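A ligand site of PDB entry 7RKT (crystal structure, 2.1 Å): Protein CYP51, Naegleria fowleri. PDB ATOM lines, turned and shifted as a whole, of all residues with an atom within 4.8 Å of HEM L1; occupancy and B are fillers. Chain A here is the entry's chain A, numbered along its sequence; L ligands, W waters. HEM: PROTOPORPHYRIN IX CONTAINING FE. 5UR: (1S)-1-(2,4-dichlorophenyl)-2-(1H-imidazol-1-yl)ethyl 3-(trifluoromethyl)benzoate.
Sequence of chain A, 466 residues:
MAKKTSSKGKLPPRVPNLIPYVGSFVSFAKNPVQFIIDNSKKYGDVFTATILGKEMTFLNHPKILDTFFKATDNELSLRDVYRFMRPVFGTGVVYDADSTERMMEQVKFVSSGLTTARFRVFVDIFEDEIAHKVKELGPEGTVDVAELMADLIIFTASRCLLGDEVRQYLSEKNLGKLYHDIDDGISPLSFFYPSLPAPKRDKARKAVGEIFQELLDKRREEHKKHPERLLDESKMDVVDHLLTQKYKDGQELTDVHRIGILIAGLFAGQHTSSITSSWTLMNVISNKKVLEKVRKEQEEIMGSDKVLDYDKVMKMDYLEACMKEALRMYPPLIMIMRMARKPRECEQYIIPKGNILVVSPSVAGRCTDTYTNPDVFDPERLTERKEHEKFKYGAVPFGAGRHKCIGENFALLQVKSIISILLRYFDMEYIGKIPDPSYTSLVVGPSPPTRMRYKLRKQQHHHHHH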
ATOM      1  N   LEU A  78     -26.961  11.809  18.226  1.00  0.00           N
ATOM      2  CA  LEU A  78     -25.741  12.398  18.749  1.00  0.00           C
ATOM      3  C   LEU A  78     -24.833  11.333  19.296  1.00  0.00           C
ATOM      4  O   LEU A  78     -23.608  11.472  19.246  1.00  0.00           O
ATOM      5  CB  LEU A  78     -26.027  13.350  19.880  1.00  0.00           C
ATOM      6  CG  LEU A  78     -26.513  14.722  19.442  1.00  0.00           C
ATOM      7  CD1 LEU A  78     -27.982  14.654  19.023  1.00  0.00           C
ATOM      8  CD2 LEU A  78     -26.312  15.714  20.576  1.00  0.00           C
ATOM      9  N   TYR A  82     -20.536  11.004  18.907  1.00  0.00           N
ATOM     10  CA  TYR A  82     -19.726  11.661  19.932  1.00  0.00           C
ATOM     11  C   TYR A  82     -19.407  10.733  21.108  1.00  0.00           C
ATOM     12  O   TYR A  82     -18.890  11.176  22.142  1.00  0.00           O
ATOM     13  CB  TYR A  82     -20.480  12.881  20.455  1.00  0.00           C
ATOM     14  CG  TYR A  82     -20.765  13.959  19.445  1.00  0.00           C
ATOM     15  CD1 TYR A  82     -19.743  14.470  18.661  1.00  0.00           C
ATOM     16  CD2 TYR A  82     -22.019  14.526  19.335  1.00  0.00           C
ATOM     17  CE1 TYR A  82     -19.979  15.498  17.757  1.00  0.00           C
ATOM     18  CE2 TYR A  82     -22.279  15.539  18.434  1.00  0.00           C
ATOM     19  CZ  TYR A  82     -21.247  16.016  17.639  1.00  0.00           C
ATOM     20  OH  TYR A  82     -21.444  17.034  16.732  1.00  0.00           O
ATOM     21  N   VAL A 107     -27.965  15.799  31.970  1.00  0.00           N
ATOM     22  CA  VAL A 107     -27.895  17.153  31.528  1.00  0.00           C
ATOM     23  C   VAL A 107     -28.681  18.052  32.467  1.00  0.00           C
ATOM     24  O   VAL A 107     -28.137  19.060  32.914  1.00  0.00           O
ATOM     25  CB  VAL A 107     -28.426  17.281  30.093  1.00  0.00           C
ATOM     26  CG1 VAL A 107     -28.679  18.730  29.712  1.00  0.00           C
ATOM     27  CG2 VAL A 107     -27.407  16.633  29.181  1.00  0.00           C
ATOM     28  N   VAL A 110     -26.914  19.295  35.587  1.00  0.00           N
ATOM     29  CA  VAL A 110     -26.019  20.413  35.407  1.00  0.00           C
ATOM     30  C   VAL A 110     -26.865  21.692  35.356  1.00  0.00           C
ATOM     31  O   VAL A 110     -26.602  22.668  36.092  1.00  0.00           O
ATOM     32  CB  VAL A 110     -25.135  20.254  34.145  1.00  0.00           C
ATOM     33  CG1 VAL A 110     -24.308  21.501  33.881  1.00  0.00           C
ATOM     34  CG2 VAL A 110     -24.215  19.052  34.319  1.00  0.00           C
ATOM     35  N   LEU A 114     -27.723  26.020  37.500  1.00  0.00           N
ATOM     36  CA  LEU A 114     -27.549  27.224  36.716  1.00  0.00           C
ATOM     37  C   LEU A 114     -28.822  28.037  36.718  1.00  0.00           C
ATOM     38  O   LEU A 114     -29.345  28.360  35.704  1.00  0.00           O
ATOM     39  CB  LEU A 114     -27.132  26.841  35.300  1.00  0.00           C
ATOM     40  CG  LEU A 114     -25.826  26.067  35.114  1.00  0.00           C
ATOM     41  CD1 LEU A 114     -25.587  25.995  33.594  1.00  0.00           C
ATOM     42  CD2 LEU A 114     -24.657  26.705  35.832  1.00  0.00           C
ATOM     43  N   LEU A 161     -19.705  25.794  39.571  1.00  0.00           N
ATOM     44  CA  LEU A 161     -20.302  24.498  39.451  1.00  0.00           C
ATOM     45  C   LEU A 161     -19.972  23.641  40.657  1.00  0.00           C
ATOM     46  O   LEU A 161     -20.860  22.889  41.107  1.00  0.00           O
ATOM     47  CB  LEU A 161     -19.805  23.809  38.179  1.00  0.00           C
ATOM     48  CG  LEU A 161     -20.030  24.627  36.882  1.00  0.00           C
ATOM     49  CD1 LEU A 161     -19.837  23.748  35.660  1.00  0.00           C
ATOM     50  CD2 LEU A 161     -21.389  25.294  36.813  1.00  0.00           C
ATOM     51  N   GLY A 265     -19.135  18.891  32.678  1.00  0.00           N
ATOM     52  CA  GLY A 265     -19.686  20.227  32.940  1.00  0.00           C
ATOM     53  C   GLY A 265     -18.671  21.347  32.819  1.00  0.00           C
ATOM     54  O   GLY A 265     -18.936  22.349  32.219  1.00  0.00           O
ATOM     55  N   ALA A 268     -17.251  21.461  29.183  1.00  0.00           N
ATOM     56  CA  ALA A 268     -18.157  22.186  28.275  1.00  0.00           C
ATOM     57  C   ALA A 268     -17.784  23.657  28.185  1.00  0.00           C
ATOM     58  O   ALA A 268     -17.413  24.173  27.103  1.00  0.00           O
ATOM     59  CB  ALA A 268     -19.611  22.055  28.719  1.00  0.00           C
ATOM     60  N   GLY A 269     -17.819  24.287  29.353  1.00  0.00           N
ATOM     61  CA  GLY A 269     -17.599  25.721  29.499  1.00  0.00           C
ATOM     62  C   GLY A 269     -16.300  25.985  30.195  1.00  0.00           C
ATOM     63  O   GLY A 269     -16.250  26.621  31.264  1.00  0.00           O
ATOM     64  N   THR A 272     -14.853  26.748  25.219  1.00  0.00           N
ATOM     65  CA  THR A 272     -15.752  27.555  24.381  1.00  0.00           C
ATOM     66  C   THR A 272     -15.962  28.977  24.931  1.00  0.00           C
ATOM     67  O   THR A 272     -15.818  29.932  24.191  1.00  0.00           O
ATOM     68  CB  THR A 272     -17.138  26.937  24.257  1.00  0.00           C
ATOM     69  OG1 THR A 272     -17.601  26.585  25.558  1.00  0.00           O
ATOM     70  CG2 THR A 272     -17.094  25.746  23.411  1.00  0.00           C
ATOM     71  N   SER A 273     -16.265  29.090  26.216  1.00  0.00           N
ATOM     72  CA  SER A 273     -16.392  30.359  26.859  1.00  0.00           C
ATOM     73  C   SER A 273     -15.064  31.135  26.918  1.00  0.00           C
ATOM     74  O   SER A 273     -15.069  32.352  26.825  1.00  0.00           O
ATOM     75  CB  SER A 273     -16.975  30.227  28.262  1.00  0.00           C
ATOM     76  OG  SER A 273     -18.200  29.508  28.253  1.00  0.00           O
ATOM     77  N   THR A 276     -14.387  32.361  23.353  1.00  0.00           N
ATOM     78  CA  THR A 276     -15.310  33.415  22.998  1.00  0.00           C
ATOM     79  C   THR A 276     -14.955  34.707  23.735  1.00  0.00           C
ATOM     80  O   THR A 276     -15.018  35.729  23.135  1.00  0.00           O
ATOM     81  CB  THR A 276     -16.761  32.978  23.221  1.00  0.00           C
ATOM     82  OG1 THR A 276     -17.002  31.839  22.393  1.00  0.00           O
ATOM     83  CG2 THR A 276     -17.755  34.080  22.864  1.00  0.00           C
ATOM     84  N   MET A 323     -20.425  40.052  22.046  1.00  0.00           N
ATOM     85  CA  MET A 323     -20.213  38.640  22.229  1.00  0.00           C
ATOM     86  C   MET A 323     -20.874  37.819  21.140  1.00  0.00           C
ATOM     87  O   MET A 323     -20.242  36.949  20.578  1.00  0.00           O
ATOM     88  CB  MET A 323     -20.679  38.177  23.592  1.00  0.00           C
ATOM     89  CG  MET A 323     -20.251  36.731  23.845  1.00  0.00           C
ATOM     90  SD  MET A 323     -20.873  36.180  25.434  1.00  0.00           S
ATOM     91  CE  MET A 323     -20.720  34.401  25.242  1.00  0.00           C
ATOM     92  N   LEU A 327     -19.210  35.256  18.200  1.00  0.00           N
ATOM     93  CA  LEU A 327     -19.730  33.906  17.943  1.00  0.00           C
ATOM     94  C   LEU A 327     -20.195  33.645  16.522  1.00  0.00           C
ATOM     95  O   LEU A 327     -20.069  32.506  16.060  1.00  0.00           O
ATOM     96  CB  LEU A 327     -20.894  33.558  18.861  1.00  0.00           C
ATOM     97  CG  LEU A 327     -20.481  33.358  20.328  1.00  0.00           C
ATOM     98  CD1 LEU A 327     -21.652  33.498  21.256  1.00  0.00           C
ATOM     99  CD2 LEU A 327     -19.803  31.990  20.496  1.00  0.00           C
ATOM    100  N   PRO A 332     -16.526  28.591  18.335  1.00  0.00           N
ATOM    101  CA  PRO A 332     -15.544  27.607  18.794  1.00  0.00           C
ATOM    102  C   PRO A 332     -15.875  26.124  18.488  1.00  0.00           C
ATOM    103  O   PRO A 332     -14.961  25.300  18.461  1.00  0.00           O
ATOM    104  CB  PRO A 332     -15.527  27.830  20.299  1.00  0.00           C
ATOM    105  CG  PRO A 332     -16.904  28.244  20.614  1.00  0.00           C
ATOM    106  CD  PRO A 332     -17.261  29.172  19.481  1.00  0.00           C
ATOM    107  N   LEU A 333     -17.160  25.799  18.303  1.00  0.00           N
ATOM    108  CA  LEU A 333     -17.587  24.520  17.755  1.00  0.00           C
ATOM    109  C   LEU A 333     -17.936  24.806  16.281  1.00  0.00           C
ATOM    110  O   LEU A 333     -19.017  25.250  15.933  1.00  0.00           O
ATOM    111  CB  LEU A 333     -18.757  23.922  18.523  1.00  0.00           C
ATOM    112  CG  LEU A 333     -18.564  23.893  20.052  1.00  0.00           C
ATOM    113  CD1 LEU A 333     -19.774  23.379  20.834  1.00  0.00           C
ATOM    114  CD2 LEU A 333     -17.306  23.126  20.423  1.00  0.00           C
ATOM    115  N   ILE A 336     -21.198  20.744  13.846  1.00  0.00           N
ATOM    116  CA  ILE A 336     -22.194  20.050  14.628  1.00  0.00           C
ATOM    117  C   ILE A 336     -22.597  18.841  13.816  1.00  0.00           C
ATOM    118  O   ILE A 336     -22.818  18.958  12.621  1.00  0.00           O
ATOM    119  CB  ILE A 336     -23.431  20.963  14.837  1.00  0.00           C
ATOM    120  CG1 ILE A 336     -23.084  22.127  15.735  1.00  0.00           C
ATOM    121  CG2 ILE A 336     -24.580  20.243  15.513  1.00  0.00           C
ATOM    122  CD1 ILE A 336     -24.119  23.238  15.672  1.00  0.00           C
ATOM    123  N   ARG A 338     -24.719  14.747  13.379  1.00  0.00           N
ATOM    124  CA  ARG A 338     -25.685  13.702  13.697  1.00  0.00           C
ATOM    125  C   ARG A 338     -25.467  12.475  12.804  1.00  0.00           C
ATOM    126  O   ARG A 338     -25.141  12.649  11.636  1.00  0.00           O
ATOM    127  CB  ARG A 338     -27.065  14.214  13.398  1.00  0.00           C
ATOM    128  CG  ARG A 338     -27.432  15.494  14.104  1.00  0.00           C
ATOM    129  CD  ARG A 338     -27.665  15.212  15.564  1.00  0.00           C
ATOM    130  NE  ARG A 338     -28.107  16.427  16.208  1.00  0.00           N
ATOM    131  CZ  ARG A 338     -27.339  17.321  16.814  1.00  0.00           C
ATOM    132  NH1 ARG A 338     -26.023  17.170  16.877  1.00  0.00           N
ATOM    133  NH2 ARG A 338     -27.908  18.401  17.359  1.00  0.00           N
ATOM    134  N   VAL A 396     -26.833  29.956  14.546  1.00  0.00           N
ATOM    135  CA  VAL A 396     -26.849  28.744  15.384  1.00  0.00           C
ATOM    136  C   VAL A 396     -25.563  28.591  16.213  1.00  0.00           C
ATOM    137  O   VAL A 396     -25.014  27.513  16.303  1.00  0.00           O
ATOM    138  CB  VAL A 396     -27.100  27.494  14.527  1.00  0.00           C
ATOM    139  CG1 VAL A 396     -28.554  27.462  14.066  1.00  0.00           C
ATOM    140  CG2 VAL A 396     -26.139  27.452  13.318  1.00  0.00           C
ATOM    141  N   PRO A 397     -25.066  29.678  16.815  1.00  0.00           N
ATOM    142  CA  PRO A 397     -23.867  29.475  17.633  1.00  0.00           C
ATOM    143  C   PRO A 397     -24.105  28.579  18.864  1.00  0.00           C
ATOM    144  O   PRO A 397     -23.230  27.848  19.253  1.00  0.00           O
ATOM    145  CB  PRO A 397     -23.498  30.900  18.056  1.00  0.00           C
ATOM    146  CG  PRO A 397     -24.781  31.642  18.039  1.00  0.00           C
ATOM    147  CD  PRO A 397     -25.603  31.039  16.955  1.00  0.00           C
ATOM    148  N   PHE A 398     -25.314  28.626  19.434  1.00  0.00           N
ATOM    149  CA  PHE A 398     -25.690  27.815  20.608  1.00  0.00           C
ATOM    150  C   PHE A 398     -26.559  26.612  20.223  1.00  0.00           C
ATOM    151  O   PHE A 398     -27.016  25.854  21.064  1.00  0.00           O
ATOM    152  CB  PHE A 398     -26.329  28.720  21.663  1.00  0.00           C
ATOM    153  CG  PHE A 398     -25.340  29.673  22.348  1.00  0.00           C
ATOM    154  CD1 PHE A 398     -24.440  29.198  23.276  1.00  0.00           C
ATOM    155  CD2 PHE A 398     -25.384  31.031  22.118  1.00  0.00           C
ATOM    156  CE1 PHE A 398     -23.581  30.060  23.944  1.00  0.00           C
ATOM    157  CE2 PHE A 398     -24.520  31.911  22.786  1.00  0.00           C
ATOM    158  CZ  PHE A 398     -23.615  31.415  23.703  1.00  0.00           C
ATOM    159  N   GLY A 399     -26.703  26.376  18.932  1.00  0.00           N
ATOM    160  CA  GLY A 399     -27.485  25.263  18.458  1.00  0.00           C
ATOM    161  C   GLY A 399     -28.935  25.664  18.368  1.00  0.00           C
ATOM    162  O   GLY A 399     -29.287  26.850  18.419  1.00  0.00           O
ATOM    163  N   ARG A 402     -33.730  20.419  19.872  1.00  0.00           N
ATOM    164  CA  ARG A 402     -33.837  19.570  21.040  1.00  0.00           C
ATOM    165  C   ARG A 402     -32.531  19.555  21.817  1.00  0.00           C
ATOM    166  O   ARG A 402     -32.532  19.299  23.023  1.00  0.00           O
ATOM    167  CB  ARG A 402     -34.301  18.189  20.596  1.00  0.00           C
ATOM    168  CG  ARG A 402     -34.462  17.124  21.670  1.00  0.00           C
ATOM    169  CD  ARG A 402     -34.776  15.752  21.040  1.00  0.00           C
ATOM    170  NE  ARG A 402     -36.194  15.630  20.646  1.00  0.00           N
ATOM    171  CZ  ARG A 402     -36.722  15.992  19.481  1.00  0.00           C
ATOM    172  NH1 ARG A 402     -35.991  16.500  18.494  1.00  0.00           N
ATOM    173  NH2 ARG A 402     -38.018  15.834  19.277  1.00  0.00           N
ATOM    174  N   HIS A 403     -31.418  19.850  21.155  1.00  0.00           N
ATOM    175  CA  HIS A 403     -30.118  19.845  21.842  1.00  0.00           C
ATOM    176  C   HIS A 403     -29.516  21.250  21.830  1.00  0.00           C
ATOM    177  O   HIS A 403     -28.330  21.386  21.714  1.00  0.00           O
ATOM    178  CB  HIS A 403     -29.211  18.830  21.183  1.00  0.00           C
ATOM    179  CG  HIS A 403     -29.753  17.451  21.209  1.00  0.00           C
ATOM    180  ND1 HIS A 403     -29.604  16.617  22.302  1.00  0.00           N
ATOM    181  CD2 HIS A 403     -30.471  16.743  20.296  1.00  0.00           C
ATOM    182  CE1 HIS A 403     -30.179  15.456  22.049  1.00  0.00           C
ATOM    183  NE2 HIS A 403     -30.723  15.522  20.856  1.00  0.00           N
ATOM    184  N   LYS A 404     -30.343  22.282  21.989  1.00  0.00           N
ATOM    185  CA  LYS A 404     -29.861  23.621  22.210  1.00  0.00           C
ATOM    186  C   LYS A 404     -28.947  23.627  23.478  1.00  0.00           C
ATOM    187  O   LYS A 404     -29.108  22.794  24.369  1.00  0.00           O
ATOM    188  CB  LYS A 404     -31.022  24.564  22.372  1.00  0.00           C
ATOM    189  CG  LYS A 404     -30.728  25.984  21.918  1.00  0.00           C
ATOM    190  CD  LYS A 404     -32.001  26.847  21.900  1.00  0.00           C
ATOM    191  CE  LYS A 404     -31.685  28.331  21.715  1.00  0.00           C
ATOM    192  NZ  LYS A 404     -30.656  28.648  20.679  1.00  0.00           N
ATOM    193  N   CYS A 405     -27.948  24.517  23.479  1.00  0.00           N
ATOM    194  CA  CYS A 405     -27.019  24.649  24.573  1.00  0.00           C
ATOM    195  C   CYS A 405     -27.739  24.952  25.869  1.00  0.00           C
ATOM    196  O   CYS A 405     -28.414  25.945  25.983  1.00  0.00           O
ATOM    197  CB  CYS A 405     -26.014  25.757  24.272  1.00  0.00           C
ATOM    198  SG  CYS A 405     -24.640  25.830  25.514  1.00  0.00           S
ATOM    199  N   ILE A 406     -27.592  24.137  26.881  1.00  0.00           N
ATOM    200  CA  ILE A 406     -28.215  24.538  28.157  1.00  0.00           C
ATOM    201  C   ILE A 406     -27.314  25.484  28.931  1.00  0.00           C
ATOM    202  O   ILE A 406     -27.748  26.046  29.906  1.00  0.00           O
ATOM    203  CB  ILE A 406     -28.674  23.305  28.978  1.00  0.00           C
ATOM    204  CG1 ILE A 406     -27.511  22.441  29.469  1.00  0.00           C
ATOM    205  CG2 ILE A 406     -29.626  22.472  28.128  1.00  0.00           C
ATOM    206  CD1 ILE A 406     -26.783  22.958  30.673  1.00  0.00           C
ATOM    207  N   GLY A 407     -26.083  25.724  28.458  1.00  0.00           N
ATOM    208  CA  GLY A 407     -25.135  26.613  29.117  1.00  0.00           C
ATOM    209  C   GLY A 407     -25.159  28.053  28.654  1.00  0.00           C
ATOM    210  O   GLY A 407     -24.404  28.854  29.161  1.00  0.00           O
ATOM    211  N   PHE A 410     -25.480  31.002  31.151  1.00  0.00           N
ATOM    212  CA  PHE A 410     -24.255  31.064  32.056  1.00  0.00           C
ATOM    213  C   PHE A 410     -23.077  31.586  31.256  1.00  0.00           C
ATOM    214  O   PHE A 410     -22.296  32.370  31.751  1.00  0.00           O
ATOM    215  CB  PHE A 410     -23.913  29.700  32.598  1.00  0.00           C
ATOM    216  CG  PHE A 410     -22.613  29.656  33.386  1.00  0.00           C
ATOM    217  CD1 PHE A 410     -22.521  30.265  34.631  1.00  0.00           C
ATOM    218  CD2 PHE A 410     -21.512  28.999  32.908  1.00  0.00           C
ATOM    219  CE1 PHE A 410     -21.321  30.215  35.368  1.00  0.00           C
ATOM    220  CE2 PHE A 410     -20.316  28.939  33.635  1.00  0.00           C
ATOM    221  CZ  PHE A 410     -20.233  29.560  34.862  1.00  0.00           C
ATOM    222  N   ALA A 411     -22.971  31.184  30.001  1.00  0.00           N
ATOM    223  CA  ALA A 411     -21.826  31.612  29.215  1.00  0.00           C
ATOM    224  C   ALA A 411     -21.833  33.106  29.001  1.00  0.00           C
ATOM    225  O   ALA A 411     -20.817  33.812  29.242  1.00  0.00           O
ATOM    226  CB  ALA A 411     -21.799  30.888  27.898  1.00  0.00           C
HETATM  227  CHA HEM L   1     -24.895  22.190  23.316  1.00  0.00           C
HETATM  228  CHB HEM L   1     -22.215  26.000  22.031  1.00  0.00           C
HETATM  229  CHC HEM L   1     -21.255  26.873  26.698  1.00  0.00           C
HETATM  230  CHD HEM L   1     -23.443  22.808  27.855  1.00  0.00           C
HETATM  231  C1A HEM L   1     -24.282  23.180  22.601  1.00  0.00           C
HETATM  232  C2A HEM L   1     -24.384  23.312  21.194  1.00  0.00           C
HETATM  233  C3A HEM L   1     -23.623  24.378  20.836  1.00  0.00           C
HETATM  234  C4A HEM L   1     -23.044  24.891  22.014  1.00  0.00           C
HETATM  235  CMA HEM L   1     -23.408  24.893  19.427  1.00  0.00           C
HETATM  236  CAA HEM L   1     -25.160  22.423  20.277  1.00  0.00           C
HETATM  237  CBA HEM L   1     -24.407  21.078  20.086  1.00  0.00           C
HETATM  238  CGA HEM L   1     -25.116  20.108  19.113  1.00  0.00           C
HETATM  239  O1A HEM L   1     -24.586  18.992  18.792  1.00  0.00           O
HETATM  240  O2A HEM L   1     -26.231  20.401  18.608  1.00  0.00           O
HETATM  241  C1B HEM L   1     -21.716  26.565  23.197  1.00  0.00           C
HETATM  242  C2B HEM L   1     -20.969  27.768  23.192  1.00  0.00           C
HETATM  243  C3B HEM L   1     -20.649  28.031  24.506  1.00  0.00           C
HETATM  244  C4B HEM L   1     -21.296  26.959  25.305  1.00  0.00           C
HETATM  245  CMB HEM L   1     -20.546  28.566  21.993  1.00  0.00           C
HETATM  246  CAB HEM L   1     -19.960  29.182  25.100  1.00  0.00           C
HETATM  247  CBB HEM L   1     -19.874  30.373  24.516  1.00  0.00           C
HETATM  248  C1C HEM L   1     -21.776  25.829  27.435  1.00  0.00           C
HETATM  249  C2C HEM L   1     -21.575  25.650  28.812  1.00  0.00           C
HETATM  250  C3C HEM L   1     -22.223  24.462  29.159  1.00  0.00           C
HETATM  251  C4C HEM L   1     -22.773  23.961  27.938  1.00  0.00           C
HETATM  252  CMC HEM L   1     -20.857  26.656  29.674  1.00  0.00           C
HETATM  253  CAC HEM L   1     -22.417  23.793  30.446  1.00  0.00           C
HETATM  254  CBC HEM L   1     -22.085  24.309  31.638  1.00  0.00           C
HETATM  255  C1D HEM L   1     -24.003  22.363  26.695  1.00  0.00           C
HETATM  256  C2D HEM L   1     -24.797  21.164  26.745  1.00  0.00           C
HETATM  257  C3D HEM L   1     -25.232  20.993  25.502  1.00  0.00           C
HETATM  258  C4D HEM L   1     -24.669  22.066  24.691  1.00  0.00           C
HETATM  259  CMD HEM L   1     -25.107  20.253  27.913  1.00  0.00           C
HETATM  260  CAD HEM L   1     -26.042  19.785  25.082  1.00  0.00           C
HETATM  261  CBD HEM L   1     -27.486  20.128  24.800  1.00  0.00           C
HETATM  262  CGD HEM L   1     -28.263  18.807  24.708  1.00  0.00           C
HETATM  263  O1D HEM L   1     -29.354  18.681  25.347  1.00  0.00           O
HETATM  264  O2D HEM L   1     -27.799  17.862  23.991  1.00  0.00           O
HETATM  265  NA  HEM L   1     -23.462  24.170  23.051  1.00  0.00           N
HETATM  266  NB  HEM L   1     -21.897  26.119  24.452  1.00  0.00           N
HETATM  267  NC  HEM L   1     -22.443  24.758  26.960  1.00  0.00           N
HETATM  268  ND  HEM L   1     -23.939  22.912  25.462  1.00  0.00           N
HETATM  269 FE   HEM L   1     -22.982  24.460  24.983  1.00  0.00          FE
HETATM  270  C4  5UR L   2     -18.539  18.448  23.217  1.00  0.00           C
HETATM  271  C8  5UR L   2     -19.812  19.114  26.173  1.00  0.00           C
HETATM  272  C9  5UR L   2     -21.047  18.570  26.777  1.00  0.00           C
HETATM  273  C10 5UR L   2     -22.007  17.968  25.978  1.00  0.00           C
HETATM  274  C11 5UR L   2     -23.124  17.394  26.581  1.00  0.00           C
HETATM  275  C14 5UR L   2     -21.246  18.607  28.153  1.00  0.00           C
HETATM  276  C15 5UR L   2     -22.576  18.077  30.293  1.00  0.00           C
HETATM  277  C17 5UR L   2     -19.265  22.760  24.524  1.00  0.00           C
HETATM  278  C18 5UR L   2     -20.203  23.654  24.975  1.00  0.00           C
HETATM  279 CL1  5UR L   2     -17.090  15.181  20.470  1.00  0.00          CL
HETATM  280  CG  5UR L   2     -17.638  16.435  21.526  1.00  0.00           C
HETATM  281  CD1 5UR L   2     -18.938  16.400  22.014  1.00  0.00           C
HETATM  282  CE1 5UR L   2     -19.382  17.415  22.849  1.00  0.00           C
HETATM  283  CE2 5UR L   2     -17.243  18.442  22.688  1.00  0.00           C
HETATM  284  CD2 5UR L   2     -16.765  17.439  21.850  1.00  0.00           C
HETATM  285 CL2  5UR L   2     -16.119  19.712  23.068  1.00  0.00          CL
HETATM  286  C   5UR L   2     -18.964  19.572  24.070  1.00  0.00           C
HETATM  287  O   5UR L   2     -19.889  19.086  24.814  1.00  0.00           O
HETATM  288  OH  5UR L   2     -18.834  19.388  26.861  1.00  0.00           O
HETATM  289  C12 5UR L   2     -23.284  17.421  27.963  1.00  0.00           C
HETATM  290  C13 5UR L   2     -22.359  18.042  28.775  1.00  0.00           C
HETATM  291  F1  5UR L   2     -21.731  18.871  31.003  1.00  0.00           F
HETATM  292  F2  5UR L   2     -23.804  18.536  30.633  1.00  0.00           F
HETATM  293  F3  5UR L   2     -22.523  16.883  30.934  1.00  0.00           F
HETATM  294  CA  5UR L   2     -19.411  20.610  23.096  1.00  0.00           C
HETATM  295  N   5UR L   2     -19.953  21.822  23.789  1.00  0.00           N
HETATM  296  N2  5UR L   2     -21.482  23.288  24.538  1.00  0.00           N
HETATM  297  C19 5UR L   2     -21.252  22.188  23.855  1.00  0.00           C
HETATM  298  O   HOH W   1     -28.446  22.072  18.901  1.00  0.00           O
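An iron atom (FE) of HEM L1 is bound by the side-chain sulfur of Cys 405 (2.2 Å).
A ring nitrogen (ND1) of His 403 is in hydrogen-bond range of an oxygen (O2D) of HEM L1 (2.8 Å).
The guanidinium group (NH2) of Arg 338 lies within salt-bridge range of an oxygen (O2A) of HEM L1 (2.9 Å).
The backbone NH (N) of Ala 268 lies close to an oxygen (OH) of 5UR L2, at 3.5 Å.
N2 of 5UR L2 is bound to FE of HEM L1 (2.0 Å).
The backbone carbonyl oxygen (O) of Phe 398 lies within hydrogen-bond range of the backbone NH (N) of Cys 405, at 2.9 Å.
The side-chain sulfur (SG) of Cys 405 lies close to the backbone NH (N) of Gly 407, at 3.3 Å.
NZ of Lys 404 sits at hydrogen-bond distance from O of Gly 399 (3.2 Å).
OG1 of Thr 272 is in hydrogen-bond range of O of Ala 268, 2.9 Å away.
O of Thr 272 is in hydrogen-bond range of OG1 of Thr 276 (2.9 Å).
Gly 265 touches HEM L1.
CB of Ala 268 touches C3C of HEM L1, 3.6 Å away.
Gly 269 touches HEM L1 (CA to CMC, 3.4 Å).
Thr 272 touches HEM L1 (OG1 to C3B, 3.5 Å).
Ser 273 touches HEM L1 (OG to CAB, 3.6 Å).
Thr 276 touches HEM L1.
Leu 327 touches HEM L1 (CD2 to CMB, 3.8 Å).
CG of Pro 332 touches CMB of HEM L1 (3.9 Å).
Leu 333 touches HEM L1.
Ile 336 touches HEM L1.
Pro 397 touches HEM L1.
Phe 398 touches HEM L1 (CE1 to C2B, 3.6 Å).
Gly 399 touches HEM L1 (N to CMA, 3.6 Å).
Arg 402 touches HEM L1.
Lys 404 touches HEM L1.
Ile 406 touches HEM L1 (CG1 to CMD, 3.6 Å).
CA of Gly 407 touches C3C of HEM L1, 3.6 Å away.
CB of Ala 411 touches CAB of HEM L1, at 3.8 Å.
Hydrophobic or aromatic side chains within 4 Å of HEM L1: Ala 268, Leu 327, Pro 332, Leu 333, Ile 336, Phe 398, His 403, Ile 406 and Ala 411.
Water W1 lies within hydrogen-bond range of an oxygen (O2A) of HEM L1 (2.8 Å) and the backbone carbonyl oxygen of His 403 (2.9 Å).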
